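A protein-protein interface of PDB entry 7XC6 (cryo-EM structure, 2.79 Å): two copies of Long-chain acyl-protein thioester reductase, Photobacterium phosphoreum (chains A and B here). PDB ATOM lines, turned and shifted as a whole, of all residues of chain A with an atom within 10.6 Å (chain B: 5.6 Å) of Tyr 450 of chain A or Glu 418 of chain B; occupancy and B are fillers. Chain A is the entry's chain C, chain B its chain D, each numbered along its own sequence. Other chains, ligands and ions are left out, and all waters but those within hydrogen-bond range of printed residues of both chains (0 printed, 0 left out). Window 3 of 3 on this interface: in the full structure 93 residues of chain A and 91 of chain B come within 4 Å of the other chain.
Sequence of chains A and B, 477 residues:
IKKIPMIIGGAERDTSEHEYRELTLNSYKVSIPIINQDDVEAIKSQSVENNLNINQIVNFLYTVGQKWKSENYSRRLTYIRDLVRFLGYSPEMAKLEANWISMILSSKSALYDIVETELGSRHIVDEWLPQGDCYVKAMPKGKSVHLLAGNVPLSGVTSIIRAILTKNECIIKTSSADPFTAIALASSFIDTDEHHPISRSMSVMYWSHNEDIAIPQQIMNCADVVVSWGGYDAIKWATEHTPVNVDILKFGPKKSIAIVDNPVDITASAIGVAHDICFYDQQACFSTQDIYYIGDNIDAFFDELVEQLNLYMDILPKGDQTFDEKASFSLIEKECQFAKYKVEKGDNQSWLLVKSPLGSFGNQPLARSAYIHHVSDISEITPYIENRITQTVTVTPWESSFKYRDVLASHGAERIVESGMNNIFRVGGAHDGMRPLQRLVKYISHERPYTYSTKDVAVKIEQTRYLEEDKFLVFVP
OD2 of Asp 133 of chain A lies within salt-bridge range of NH2 of Arg 426 of chain B, at 3.4 Å. O of Ser 445 of chain A lies within hydrogen-bond range of N of Ile 416 of chain B. A ring nitrogen (NE2) of His 446 of chain A is in hydrogen-bond range of the indole nitrogen (NE1) of Trp 398 of chain B (3.3 Å). O of Glu 447 of chain A lies within hydrogen-bond range of NE1 of Trp 398 of chain B, at 2.9 Å. N of Glu 447 of chain A lies within hydrogen-bond range of O of Ile 416 of chain B (2.8 Å). The side-chain carboxylate of Glu 447 of chain A sits at hydrogen-bond distance from the backbone NH of Arg 426 of chain B, at 3.2 Å. The backbone carbonyl oxygen (O) of Arg 448 of chain A sits at hydrogen-bond distance from the guanidinium group (NH1) of Arg 426 of chain B (2.9 Å). NH1 of Arg 426 of chain B sits at hydrogen-bond distance from O of Pro 449 of chain A, 2.8 Å away. The backbone NH (N) of Tyr 450 of chain A sits close to the side-chain carboxylate (OE1) of Glu 418 of chain B (3.4 Å). The guanidinium group (NH2) of Arg 426 of chain B is in hydrogen-bond range of the backbone carbonyl oxygen (O) of Tyr 452 of chain A (2.6 Å). NH2 of Arg 426 of chain B is in hydrogen-bond range of O of Ser 453 of chain A, 3.4 Å away. The side-chain amide nitrogen (NE2) of Gln 463 of chain A is in hydrogen-bond range of the backbone carbonyl oxygen (O) of Gly 420 of chain B (2.8 Å).
Printed residues of chain B within 4 Å of Asp 133 of chain A: Arg 426. Printed residues of chain B within 4 Å of Glu 447 of chain A: Trp 398 (2.9 Å), Ile 416 (2.8 Å), Val 417 (3.7 Å) and Arg 426 (3.2 Å). Of the printed residues of chain B, Thr 454 of chain A touches Arg 426. Val 417 of chain B touches one residue of chain A. Glu 418 of chain B touches just these residues of chain A: Pro 449 and Tyr 450. Of chain A, only Gln 463 comes within 4 Å of Gly 420 of chain B. Of chain A, only Tyr 450 and Ile 461 come within 4 Å of Met 421 of chain B. The nearest residue of chain B that does not touch Tyr 450 of chain A is Arg 426 of chain B (4.6 Å).
Of the 23 printed residues of chain A, 13 touch a printed residue of chain B. Printed residues of chain A that touch a printed residue of chain B: Asp 133, Cys 134, Ser 445, His 446, Glu 447, Arg 448, Pro 449, Tyr 450, Tyr 452, Ser 453, Thr 454, Ile 461 and Gln 463. Hydrophobic or aromatic side chains of chain A that line the printed part of chain B: His 446, Pro 449, Tyr 450 and Ile 461. Hydrophobic or aromatic side chains of chain B that line the printed part of chain A: Trp 398, Ile 416, Val 417 and Met 421. Along chain B the printed residues that touch a printed residue of chain A span positions 398 to 426. Among the printed residues, Asp or Glu carboxylates within 4 Å of a Lys or Arg side-chain nitrogen of the other chain: Asp 133 of chain A with Arg 426 of chain B (3.4 Å).
O of Asp 133 of chain A lies close to N of Arg 448 of chain A (3.5 Å). OG of Ser 445 of chain A lies close to OE2 of Glu 447 of chain A. The side-chain hydroxyl of Thr 454 of chain A is in hydrogen-bond range of the backbone NH of Val 457 of chain A, 3.5 Å away.
CD2 of His 446 of chain A touches O of Ile 416 of chain B (3.4 Å). OE2 of Glu 418 of chain B touches CB of Pro 449 of chain A, 3.3 Å away. N of Thr 454 of chain A touches NH2 of Arg 426 of chain B, at 3.97 Å.
No position is printed for both chains. Of the 21 pairs that touch across the chains among the printed residues, none has its exchanged pair printed and touching as well.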
ATOM      1  N   ASP A 133      15.283 -25.679  17.104  1.00  0.00           N
ATOM      2  CA  ASP A 133      14.912 -25.820  15.695  1.00  0.00           C
ATOM      3  C   ASP A 133      15.969 -26.565  14.880  1.00  0.00           C
ATOM      4  O   ASP A 133      15.921 -26.556  13.650  1.00  0.00           O
ATOM      5  CB  ASP A 133      14.640 -24.456  15.054  1.00  0.00           C
ATOM      6  CG  ASP A 133      13.262 -23.928  15.368  1.00  0.00           C
ATOM      7  OD1 ASP A 133      12.491 -24.633  16.047  1.00  0.00           O
ATOM      8  OD2 ASP A 133      12.948 -22.800  14.936  1.00  0.00           O
ATOM      9  N   CYS A 134      16.917 -27.228  15.537  1.00  0.00           N
ATOM     10  CA  CYS A 134      18.045 -27.839  14.847  1.00  0.00           C
ATOM     11  C   CYS A 134      18.628 -28.935  15.724  1.00  0.00           C
ATOM     12  O   CYS A 134      18.322 -29.038  16.912  1.00  0.00           O
ATOM     13  CB  CYS A 134      19.127 -26.807  14.512  1.00  0.00           C
ATOM     14  SG  CYS A 134      18.825 -25.765  13.076  1.00  0.00           S
ATOM     15  N   SER A 445      24.920 -28.268  11.363  1.00  0.00           N
ATOM     16  CA  SER A 445      23.527 -28.074  11.724  1.00  0.00           C
ATOM     17  C   SER A 445      22.637 -28.950  10.859  1.00  0.00           C
ATOM     18  O   SER A 445      22.726 -28.915   9.630  1.00  0.00           O
ATOM     19  CB  SER A 445      23.138 -26.604  11.568  1.00  0.00           C
ATOM     20  OG  SER A 445      22.067 -26.459  10.660  1.00  0.00           O
ATOM     21  N   HIS A 446      21.776 -29.721  11.505  1.00  0.00           N
ATOM     22  CA  HIS A 446      20.787 -30.573  10.864  1.00  0.00           C
ATOM     23  C   HIS A 446      19.434 -29.963  11.209  1.00  0.00           C
ATOM     24  O   HIS A 446      18.904 -30.171  12.300  1.00  0.00           O
ATOM     25  CB  HIS A 446      20.925 -32.004  11.350  1.00  0.00           C
ATOM     26  CG  HIS A 446      19.842 -32.915  10.875  1.00  0.00           C
ATOM     27  ND1 HIS A 446      19.351 -33.945  11.644  1.00  0.00           N
ATOM     28  CD2 HIS A 446      19.156 -32.956   9.710  1.00  0.00           C
ATOM     29  CE1 HIS A 446      18.409 -34.581  10.975  1.00  0.00           C
ATOM     30  NE2 HIS A 446      18.271 -34.000   9.799  1.00  0.00           N
ATOM     31  N   GLU A 447      18.904 -29.166  10.291  1.00  0.00           N
ATOM     32  CA  GLU A 447      17.710 -28.381  10.557  1.00  0.00           C
ATOM     33  C   GLU A 447      16.461 -29.224  10.356  1.00  0.00           C
ATOM     34  O   GLU A 447      16.374 -30.017   9.415  1.00  0.00           O
ATOM     35  CB  GLU A 447      17.691 -27.157   9.650  1.00  0.00           C
ATOM     36  CG  GLU A 447      19.060 -26.518   9.536  1.00  0.00           C
ATOM     37  CD  GLU A 447      19.021 -25.105   9.011  1.00  0.00           C
ATOM     38  OE1 GLU A 447      17.978 -24.701   8.461  1.00  0.00           O
ATOM     39  OE2 GLU A 447      20.041 -24.398   9.146  1.00  0.00           O
ATOM     40  N   ARG A 448      15.491 -29.053  11.242  1.00  0.00           N
ATOM     41  CA  ARG A 448      14.338 -29.936  11.220  1.00  0.00           C
ATOM     42  C   ARG A 448      13.264 -29.412  10.271  1.00  0.00           C
ATOM     43  O   ARG A 448      13.270 -28.235   9.906  1.00  0.00           O
ATOM     44  CB  ARG A 448      13.800 -30.122  12.638  1.00  0.00           C
ATOM     45  CG  ARG A 448      13.845 -28.934  13.536  1.00  0.00           C
ATOM     46  CD  ARG A 448      13.175 -29.304  14.842  1.00  0.00           C
ATOM     47  NE  ARG A 448      14.128 -29.542  15.918  1.00  0.00           N
ATOM     48  CZ  ARG A 448      13.960 -30.450  16.871  1.00  0.00           C
ATOM     49  NH1 ARG A 448      12.880 -31.215  16.879  1.00  0.00           N
ATOM     50  NH2 ARG A 448      14.874 -30.597  17.816  1.00  0.00           N
ATOM     51  N   PRO A 449      12.329 -30.260   9.841  1.00  0.00           N
ATOM     52  CA  PRO A 449      11.588 -29.996   8.606  1.00  0.00           C
ATOM     53  C   PRO A 449      10.569 -28.872   8.756  1.00  0.00           C
ATOM     54  O   PRO A 449      10.461 -28.217   9.787  1.00  0.00           O
ATOM     55  CB  PRO A 449      10.895 -31.328   8.339  1.00  0.00           C
ATOM     56  CG  PRO A 449      10.658 -31.881   9.660  1.00  0.00           C
ATOM     57  CD  PRO A 449      11.817 -31.473  10.506  1.00  0.00           C
ATOM     58  N   TYR A 450       9.809 -28.668   7.679  1.00  0.00           N
ATOM     59  CA  TYR A 450       8.852 -27.573   7.626  1.00  0.00           C
ATOM     60  C   TYR A 450       7.673 -27.800   8.560  1.00  0.00           C
ATOM     61  O   TYR A 450       7.021 -26.836   8.971  1.00  0.00           O
ATOM     62  CB  TYR A 450       8.368 -27.382   6.189  1.00  0.00           C
ATOM     63  CG  TYR A 450       7.253 -28.317   5.791  1.00  0.00           C
ATOM     64  CD1 TYR A 450       7.522 -29.620   5.411  1.00  0.00           C
ATOM     65  CD2 TYR A 450       5.933 -27.895   5.786  1.00  0.00           C
ATOM     66  CE1 TYR A 450       6.512 -30.479   5.048  1.00  0.00           C
ATOM     67  CE2 TYR A 450       4.916 -28.748   5.426  1.00  0.00           C
ATOM     68  CZ  TYR A 450       5.211 -30.038   5.057  1.00  0.00           C
ATOM     69  OH  TYR A 450       4.200 -30.891   4.694  1.00  0.00           O
ATOM     70  N   THR A 451       7.377 -29.054   8.900  1.00  0.00           N
ATOM     71  CA  THR A 451       6.282 -29.322   9.822  1.00  0.00           C
ATOM     72  C   THR A 451       6.582 -28.825  11.227  1.00  0.00           C
ATOM     73  O   THR A 451       5.654 -28.665  12.026  1.00  0.00           O
ATOM     74  CB  THR A 451       5.966 -30.815   9.856  1.00  0.00           C
ATOM     75  OG1 THR A 451       7.179 -31.558  10.019  1.00  0.00           O
ATOM     76  CG2 THR A 451       5.294 -31.239   8.572  1.00  0.00           C
ATOM     77  N   TYR A 452       7.850 -28.585  11.548  1.00  0.00           N
ATOM     78  CA  TYR A 452       8.241 -28.005  12.826  1.00  0.00           C
ATOM     79  C   TYR A 452       8.277 -26.491  12.671  1.00  0.00           C
ATOM     80  O   TYR A 452       9.198 -25.945  12.058  1.00  0.00           O
ATOM     81  CB  TYR A 452       9.596 -28.547  13.267  1.00  0.00           C
ATOM     82  CG  TYR A 452       9.816 -28.502  14.758  1.00  0.00           C
ATOM     83  CD1 TYR A 452      10.391 -27.397  15.360  1.00  0.00           C
ATOM     84  CD2 TYR A 452       9.447 -29.567  15.560  1.00  0.00           C
ATOM     85  CE1 TYR A 452      10.595 -27.357  16.719  1.00  0.00           C
ATOM     86  CE2 TYR A 452       9.645 -29.534  16.918  1.00  0.00           C
ATOM     87  CZ  TYR A 452      10.217 -28.428  17.493  1.00  0.00           C
ATOM     88  OH  TYR A 452      10.414 -28.396  18.852  1.00  0.00           O
ATOM     89  N   SER A 453       7.278 -25.815  13.226  1.00  0.00           N
ATOM     90  CA  SER A 453       7.147 -24.381  13.045  1.00  0.00           C
ATOM     91  C   SER A 453       8.132 -23.633  13.936  1.00  0.00           C
ATOM     92  O   SER A 453       8.757 -24.196  14.837  1.00  0.00           O
ATOM     93  CB  SER A 453       5.723 -23.933  13.353  1.00  0.00           C
ATOM     94  OG  SER A 453       4.783 -24.824  12.790  1.00  0.00           O
ATOM     95  N   THR A 454       8.268 -22.340  13.673  1.00  0.00           N
ATOM     96  CA  THR A 454       9.102 -21.484  14.497  1.00  0.00           C
ATOM     97  C   THR A 454       8.322 -21.031  15.729  1.00  0.00           C
ATOM     98  O   THR A 454       7.143 -21.349  15.905  1.00  0.00           O
ATOM     99  CB  THR A 454       9.607 -20.298  13.682  1.00  0.00           C
ATOM    100  OG1 THR A 454       8.537 -19.375  13.467  1.00  0.00           O
ATOM    101  CG2 THR A 454      10.128 -20.768  12.342  1.00  0.00           C
ATOM    102  N   LYS A 455       8.989 -20.287  16.604  1.00  0.00           N
ATOM    103  CA  LYS A 455       8.363 -19.811  17.830  1.00  0.00           C
ATOM    104  C   LYS A 455       7.527 -18.557  17.628  1.00  0.00           C
ATOM    105  O   LYS A 455       6.918 -18.081  18.590  1.00  0.00           O
ATOM    106  CB  LYS A 455       9.424 -19.528  18.894  1.00  0.00           C
ATOM    107  CG  LYS A 455      10.285 -20.707  19.276  1.00  0.00           C
ATOM    108  CD  LYS A 455      11.159 -20.336  20.456  1.00  0.00           C
ATOM    109  CE  LYS A 455      11.753 -21.552  21.120  1.00  0.00           C
ATOM    110  NZ  LYS A 455      12.465 -21.184  22.371  1.00  0.00           N
ATOM    111  N   VAL A 457       5.571 -17.842  14.357  1.00  0.00           N
ATOM    112  CA  VAL A 457       4.621 -17.878  13.257  1.00  0.00           C
ATOM    113  C   VAL A 457       3.489 -18.860  13.526  1.00  0.00           C
ATOM    114  O   VAL A 457       2.321 -18.543  13.299  1.00  0.00           O
ATOM    115  CB  VAL A 457       5.335 -18.197  11.926  1.00  0.00           C
ATOM    116  CG1 VAL A 457       4.347 -18.184  10.783  1.00  0.00           C
ATOM    117  CG2 VAL A 457       6.433 -17.184  11.677  1.00  0.00           C
ATOM    118  N   ALA A 458       3.818 -20.059  14.008  1.00  0.00           N
ATOM    119  CA  ALA A 458       2.839 -21.109  14.287  1.00  0.00           C
ATOM    120  C   ALA A 458       2.156 -21.597  13.017  1.00  0.00           C
ATOM    121  O   ALA A 458       1.015 -22.057  13.053  1.00  0.00           O
ATOM    122  CB  ALA A 458       1.792 -20.663  15.313  1.00  0.00           C
ATOM    123  N   VAL A 459       2.852 -21.497  11.890  1.00  0.00           N
ATOM    124  CA  VAL A 459       2.356 -21.945  10.597  1.00  0.00           C
ATOM    125  C   VAL A 459       3.433 -22.807   9.961  1.00  0.00           C
ATOM    126  O   VAL A 459       4.607 -22.425   9.951  1.00  0.00           O
ATOM    127  CB  VAL A 459       2.000 -20.760   9.680  1.00  0.00           C
ATOM    128  CG1 VAL A 459       1.589 -21.252   8.313  1.00  0.00           C
ATOM    129  CG2 VAL A 459       0.897 -19.929  10.295  1.00  0.00           C
ATOM    130  N   LYS A 460       3.040 -23.972   9.452  1.00  0.00           N
ATOM    131  CA  LYS A 460       3.989 -24.834   8.764  1.00  0.00           C
ATOM    132  C   LYS A 460       4.587 -24.100   7.574  1.00  0.00           C
ATOM    133  O   LYS A 460       3.890 -23.390   6.845  1.00  0.00           O
ATOM    134  CB  LYS A 460       3.302 -26.119   8.315  1.00  0.00           C
ATOM    135  CG  LYS A 460       2.872 -26.994   9.469  1.00  0.00           C
ATOM    136  CD  LYS A 460       2.269 -28.295   8.995  1.00  0.00           C
ATOM    137  CE  LYS A 460       1.565 -29.003  10.135  1.00  0.00           C
ATOM    138  NZ  LYS A 460       1.172 -30.388   9.770  1.00  0.00           N
ATOM    139  N   ILE A 461       5.890 -24.273   7.380  1.00  0.00           N
ATOM    140  CA  ILE A 461       6.648 -23.424   6.448  1.00  0.00           C
ATOM    141  C   ILE A 461       6.525 -24.069   5.075  1.00  0.00           C
ATOM    142  O   ILE A 461       7.376 -24.834   4.620  1.00  0.00           O
ATOM    143  CB  ILE A 461       8.099 -23.244   6.892  1.00  0.00           C
ATOM    144  CG1 ILE A 461       8.149 -22.883   8.375  1.00  0.00           C
ATOM    145  CG2 ILE A 461       8.767 -22.174   6.064  1.00  0.00           C
ATOM    146  CD1 ILE A 461       9.495 -23.082   9.006  1.00  0.00           C
ATOM    147  N   GLU A 462       5.443 -23.734   4.386  1.00  0.00           N
ATOM    148  CA  GLU A 462       5.192 -24.189   3.023  1.00  0.00           C
ATOM    149  C   GLU A 462       5.343 -22.975   2.115  1.00  0.00           C
ATOM    150  O   GLU A 462       4.371 -22.284   1.813  1.00  0.00           O
ATOM    151  CB  GLU A 462       3.814 -24.811   2.899  1.00  0.00           C
ATOM    152  CG  GLU A 462       3.428 -25.681   4.071  1.00  0.00           C
ATOM    153  CD  GLU A 462       2.164 -26.466   3.813  1.00  0.00           C
ATOM    154  OE1 GLU A 462       1.818 -26.664   2.632  1.00  0.00           O
ATOM    155  OE2 GLU A 462       1.513 -26.885   4.791  1.00  0.00           O
ATOM    156  N   GLN A 463       6.573 -22.721   1.674  1.00  0.00           N
ATOM    157  CA  GLN A 463       6.837 -21.500   0.924  1.00  0.00           C
ATOM    158  C   GLN A 463       6.223 -21.542  -0.467  1.00  0.00           C
ATOM    159  O   GLN A 463       5.790 -20.505  -0.979  1.00  0.00           O
ATOM    160  CB  GLN A 463       8.340 -21.257   0.844  1.00  0.00           C
ATOM    161  CG  GLN A 463       9.063 -21.518   2.147  1.00  0.00           C
ATOM    162  CD  GLN A 463      10.480 -21.007   2.131  1.00  0.00           C
ATOM    163  OE1 GLN A 463      10.738 -19.875   1.730  1.00  0.00           O
ATOM    164  NE2 GLN A 463      11.414 -21.841   2.564  1.00  0.00           N
ATOM    165  N   THR A 464       6.157 -22.720  -1.085  1.00  0.00           N
ATOM    166  CA  THR A 464       5.544 -22.821  -2.405  1.00  0.00           C
ATOM    167  C   THR A 464       4.041 -22.594  -2.327  1.00  0.00           C
ATOM    168  O   THR A 464       3.469 -21.859  -3.141  1.00  0.00           O
ATOM    169  CB  THR A 464       5.844 -24.185  -3.021  1.00  0.00           C
ATOM    170  OG1 THR A 464       7.257 -24.408  -3.020  1.00  0.00           O
ATOM    171  CG2 THR A 464       5.330 -24.249  -4.444  1.00  0.00           C
ATOM    172  N   ARG A 465       3.387 -23.228  -1.352  1.00  0.00           N
ATOM    173  CA  ARG A 465       1.945 -23.084  -1.204  1.00  0.00           C
ATOM    174  C   ARG A 465       1.549 -21.629  -1.011  1.00  0.00           C
ATOM    175  O   ARG A 465       0.535 -21.177  -1.552  1.00  0.00           O
ATOM    176  CB  ARG A 465       1.454 -23.930  -0.034  1.00  0.00           C
ATOM    177  CG  ARG A 465      -0.039 -23.860   0.188  1.00  0.00           C
ATOM    178  CD  ARG A 465      -0.428 -24.493   1.502  1.00  0.00           C
ATOM    179  NE  ARG A 465      -1.512 -23.769   2.153  1.00  0.00           N
ATOM    180  CZ  ARG A 465      -2.001 -24.082   3.347  1.00  0.00           C
ATOM    181  NH1 ARG A 465      -2.990 -23.370   3.867  1.00  0.00           N
ATOM    182  NH2 ARG A 465      -1.504 -25.109   4.017  1.00  0.00           N
ATOM    183  N   TYR A 466       2.339 -20.878  -0.255  1.00  0.00           N
ATOM    184  CA  TYR A 466       2.029 -19.485   0.015  1.00  0.00           C
ATOM    185  C   TYR A 466       2.555 -18.542  -1.055  1.00  0.00           C
ATOM    186  O   TYR A 466       2.097 -17.398  -1.125  1.00  0.00           O
ATOM    187  CB  TYR A 466       2.581 -19.091   1.384  1.00  0.00           C
ATOM    188  CG  TYR A 466       1.916 -19.847   2.505  1.00  0.00           C
ATOM    189  CD1 TYR A 466       0.543 -20.025   2.520  1.00  0.00           C
ATOM    190  CD2 TYR A 466       2.658 -20.405   3.531  1.00  0.00           C
ATOM    191  CE1 TYR A 466      -0.071 -20.721   3.530  1.00  0.00           C
ATOM    192  CE2 TYR A 466       2.050 -21.106   4.546  1.00  0.00           C
ATOM    193  CZ  TYR A 466       0.685 -21.260   4.540  1.00  0.00           C
ATOM    194  OH  TYR A 466       0.067 -21.956   5.549  1.00  0.00           O
ATOM    195  N   ASP B 276      14.230 -24.986  -3.976  1.00  0.00           N
ATOM    196  CA  ASP B 276      15.653 -24.751  -3.756  1.00  0.00           C
ATOM    197  C   ASP B 276      16.367 -24.351  -5.036  1.00  0.00           C
ATOM    198  O   ASP B 276      17.336 -23.588  -4.990  1.00  0.00           O
ATOM    199  CB  ASP B 276      16.328 -25.988  -3.177  1.00  0.00           C
ATOM    200  CG  ASP B 276      15.725 -26.423  -1.874  1.00  0.00           C
ATOM    201  OD1 ASP B 276      15.086 -25.592  -1.199  1.00  0.00           O
ATOM    202  OD2 ASP B 276      15.917 -27.599  -1.513  1.00  0.00           O
ATOM    203  N   THR B 394      20.869 -30.688   1.327  1.00  0.00           N
ATOM    204  CA  THR B 394      19.433 -30.941   1.325  1.00  0.00           C
ATOM    205  C   THR B 394      19.065 -32.408   1.110  1.00  0.00           C
ATOM    206  O   THR B 394      19.529 -33.042   0.160  1.00  0.00           O
ATOM    207  CB  THR B 394      18.808 -30.081   0.223  1.00  0.00           C
ATOM    208  OG1 THR B 394      18.530 -28.766   0.709  1.00  0.00           O
ATOM    209  CG2 THR B 394      17.574 -30.704  -0.325  1.00  0.00           C
ATOM    210  N   VAL B 395      18.249 -32.957   2.011  1.00  0.00           N
ATOM    211  CA  VAL B 395      17.778 -34.337   1.951  1.00  0.00           C
ATOM    212  C   VAL B 395      16.262 -34.303   1.905  1.00  0.00           C
ATOM    213  O   VAL B 395      15.629 -33.674   2.757  1.00  0.00           O
ATOM    214  CB  VAL B 395      18.262 -35.165   3.153  1.00  0.00           C
ATOM    215  CG1 VAL B 395      17.856 -36.611   2.989  1.00  0.00           C
ATOM    216  CG2 VAL B 395      19.757 -35.059   3.299  1.00  0.00           C
ATOM    217  N   THR B 396      15.681 -34.964   0.913  1.00  0.00           N
ATOM    218  CA  THR B 396      14.293 -34.643   0.622  1.00  0.00           C
ATOM    219  C   THR B 396      13.289 -35.330   1.546  1.00  0.00           C
ATOM    220  O   THR B 396      12.454 -34.636   2.140  1.00  0.00           O
ATOM    221  CB  THR B 396      13.980 -34.922  -0.841  1.00  0.00           C
ATOM    222  OG1 THR B 396      15.023 -34.380  -1.657  1.00  0.00           O
ATOM    223  CG2 THR B 396      12.742 -34.209  -1.178  1.00  0.00           C
ATOM    224  N   TRP B 398      12.811 -36.095   4.952  1.00  0.00           N
ATOM    225  CA  TRP B 398      13.646 -35.635   6.057  1.00  0.00           C
ATOM    226  C   TRP B 398      14.049 -36.768   6.992  1.00  0.00           C
ATOM    227  O   TRP B 398      15.111 -36.700   7.616  1.00  0.00           O
ATOM    228  CB  TRP B 398      12.943 -34.532   6.843  1.00  0.00           C
ATOM    229  CG  TRP B 398      13.828 -33.902   7.875  1.00  0.00           C
ATOM    230  CD1 TRP B 398      14.876 -33.059   7.654  1.00  0.00           C
ATOM    231  CD2 TRP B 398      13.748 -34.075   9.291  1.00  0.00           C
ATOM    232  NE1 TRP B 398      15.450 -32.694   8.846  1.00  0.00           N
ATOM    233  CE2 TRP B 398      14.773 -33.305   9.867  1.00  0.00           C
ATOM    234  CE3 TRP B 398      12.903 -34.804  10.129  1.00  0.00           C
ATOM    235  CZ2 TRP B 398      14.979 -33.247  11.237  1.00  0.00           C
ATOM    236  CZ3 TRP B 398      13.106 -34.741  11.485  1.00  0.00           C
ATOM    237  CH2 TRP B 398      14.132 -33.966  12.028  1.00  0.00           C
ATOM    238  N   ILE B 416      22.166 -29.771   6.873  1.00  0.00           N
ATOM    239  CA  ILE B 416      21.269 -30.788   6.340  1.00  0.00           C
ATOM    240  C   ILE B 416      19.846 -30.306   6.580  1.00  0.00           C
ATOM    241  O   ILE B 416      19.429 -30.159   7.731  1.00  0.00           O
ATOM    242  CB  ILE B 416      21.484 -32.165   6.987  1.00  0.00           C
ATOM    243  CG1 ILE B 416      22.889 -32.686   6.698  1.00  0.00           C
ATOM    244  CG2 ILE B 416      20.470 -33.151   6.467  1.00  0.00           C
ATOM    245  CD1 ILE B 416      23.811 -32.637   7.878  1.00  0.00           C
ATOM    246  N   VAL B 417      19.105 -30.054   5.503  1.00  0.00           N
ATOM    247  CA  VAL B 417      17.778 -29.464   5.578  1.00  0.00           C
ATOM    248  C   VAL B 417      16.797 -30.338   4.798  1.00  0.00           C
ATOM    249  O   VAL B 417      17.146 -31.407   4.305  1.00  0.00           O
ATOM    250  CB  VAL B 417      17.759 -28.008   5.073  1.00  0.00           C
ATOM    251  CG1 VAL B 417      18.734 -27.167   5.865  1.00  0.00           C
ATOM    252  CG2 VAL B 417      18.106 -27.953   3.621  1.00  0.00           C
ATOM    253  N   GLU B 418      15.554 -29.865   4.694  1.00  0.00           N
ATOM    254  CA  GLU B 418      14.418 -30.680   4.279  1.00  0.00           C
ATOM    255  C   GLU B 418      13.956 -30.418   2.846  1.00  0.00           C
ATOM    256  O   GLU B 418      12.892 -30.902   2.455  1.00  0.00           O
ATOM    257  CB  GLU B 418      13.249 -30.460   5.238  1.00  0.00           C
ATOM    258  CG  GLU B 418      12.202 -31.550   5.201  1.00  0.00           C
ATOM    259  CD  GLU B 418      10.811 -31.003   5.015  1.00  0.00           C
ATOM    260  OE1 GLU B 418      10.686 -29.820   4.639  1.00  0.00           O
ATOM    261  OE2 GLU B 418       9.840 -31.756   5.238  1.00  0.00           O
ATOM    262  N   SER B 419      14.716 -29.662   2.064  1.00  0.00           N
ATOM    263  CA  SER B 419      14.498 -29.330   0.658  1.00  0.00           C
ATOM    264  C   SER B 419      13.453 -28.247   0.438  1.00  0.00           C
ATOM    265  O   SER B 419      13.358 -27.744  -0.667  1.00  0.00           O
ATOM    266  CB  SER B 419      14.089 -30.540  -0.202  1.00  0.00           C
ATOM    267  OG  SER B 419      14.819 -31.690   0.147  1.00  0.00           O
ATOM    268  N   GLY B 420      12.702 -27.833   1.440  1.00  0.00           N
ATOM    269  CA  GLY B 420      11.813 -26.714   1.220  1.00  0.00           C
ATOM    270  C   GLY B 420      12.292 -25.581   2.087  1.00  0.00           C
ATOM    271  O   GLY B 420      11.605 -24.576   2.284  1.00  0.00           O
ATOM    272  N   MET B 421      13.506 -25.756   2.604  1.00  0.00           N
ATOM    273  CA  MET B 421      13.999 -24.949   3.710  1.00  0.00           C
ATOM    274  C   MET B 421      15.440 -24.509   3.501  1.00  0.00           C
ATOM    275  O   MET B 421      16.102 -24.126   4.469  1.00  0.00           O
ATOM    276  CB  MET B 421      13.895 -25.740   5.014  1.00  0.00           C
ATOM    277  CG  MET B 421      12.515 -26.293   5.307  1.00  0.00           C
ATOM    278  SD  MET B 421      11.419 -25.026   5.933  1.00  0.00           S
ATOM    279  CE  MET B 421      12.228 -24.679   7.487  1.00  0.00           C
ATOM    280  N   ARG B 426      17.657 -21.880   9.895  1.00  0.00           N
ATOM    281  CA  ARG B 426      16.825 -21.999  11.080  1.00  0.00           C
ATOM    282  C   ARG B 426      17.600 -21.608  12.327  1.00  0.00           C
ATOM    283  O   ARG B 426      18.819 -21.770  12.409  1.00  0.00           O
ATOM    284  CB  ARG B 426      16.291 -23.421  11.222  1.00  0.00           C
ATOM    285  CG  ARG B 426      15.207 -23.773  10.231  1.00  0.00           C
ATOM    286  CD  ARG B 426      14.430 -24.974  10.703  1.00  0.00           C
ATOM    287  NE  ARG B 426      13.422 -24.596  11.684  1.00  0.00           N
ATOM    288  CZ  ARG B 426      12.173 -25.042  11.684  1.00  0.00           C
ATOM    289  NH1 ARG B 426      11.773 -25.897  10.758  1.00  0.00           N
ATOM    290  NH2 ARG B 426      11.328 -24.641  12.616  1.00  0.00           N
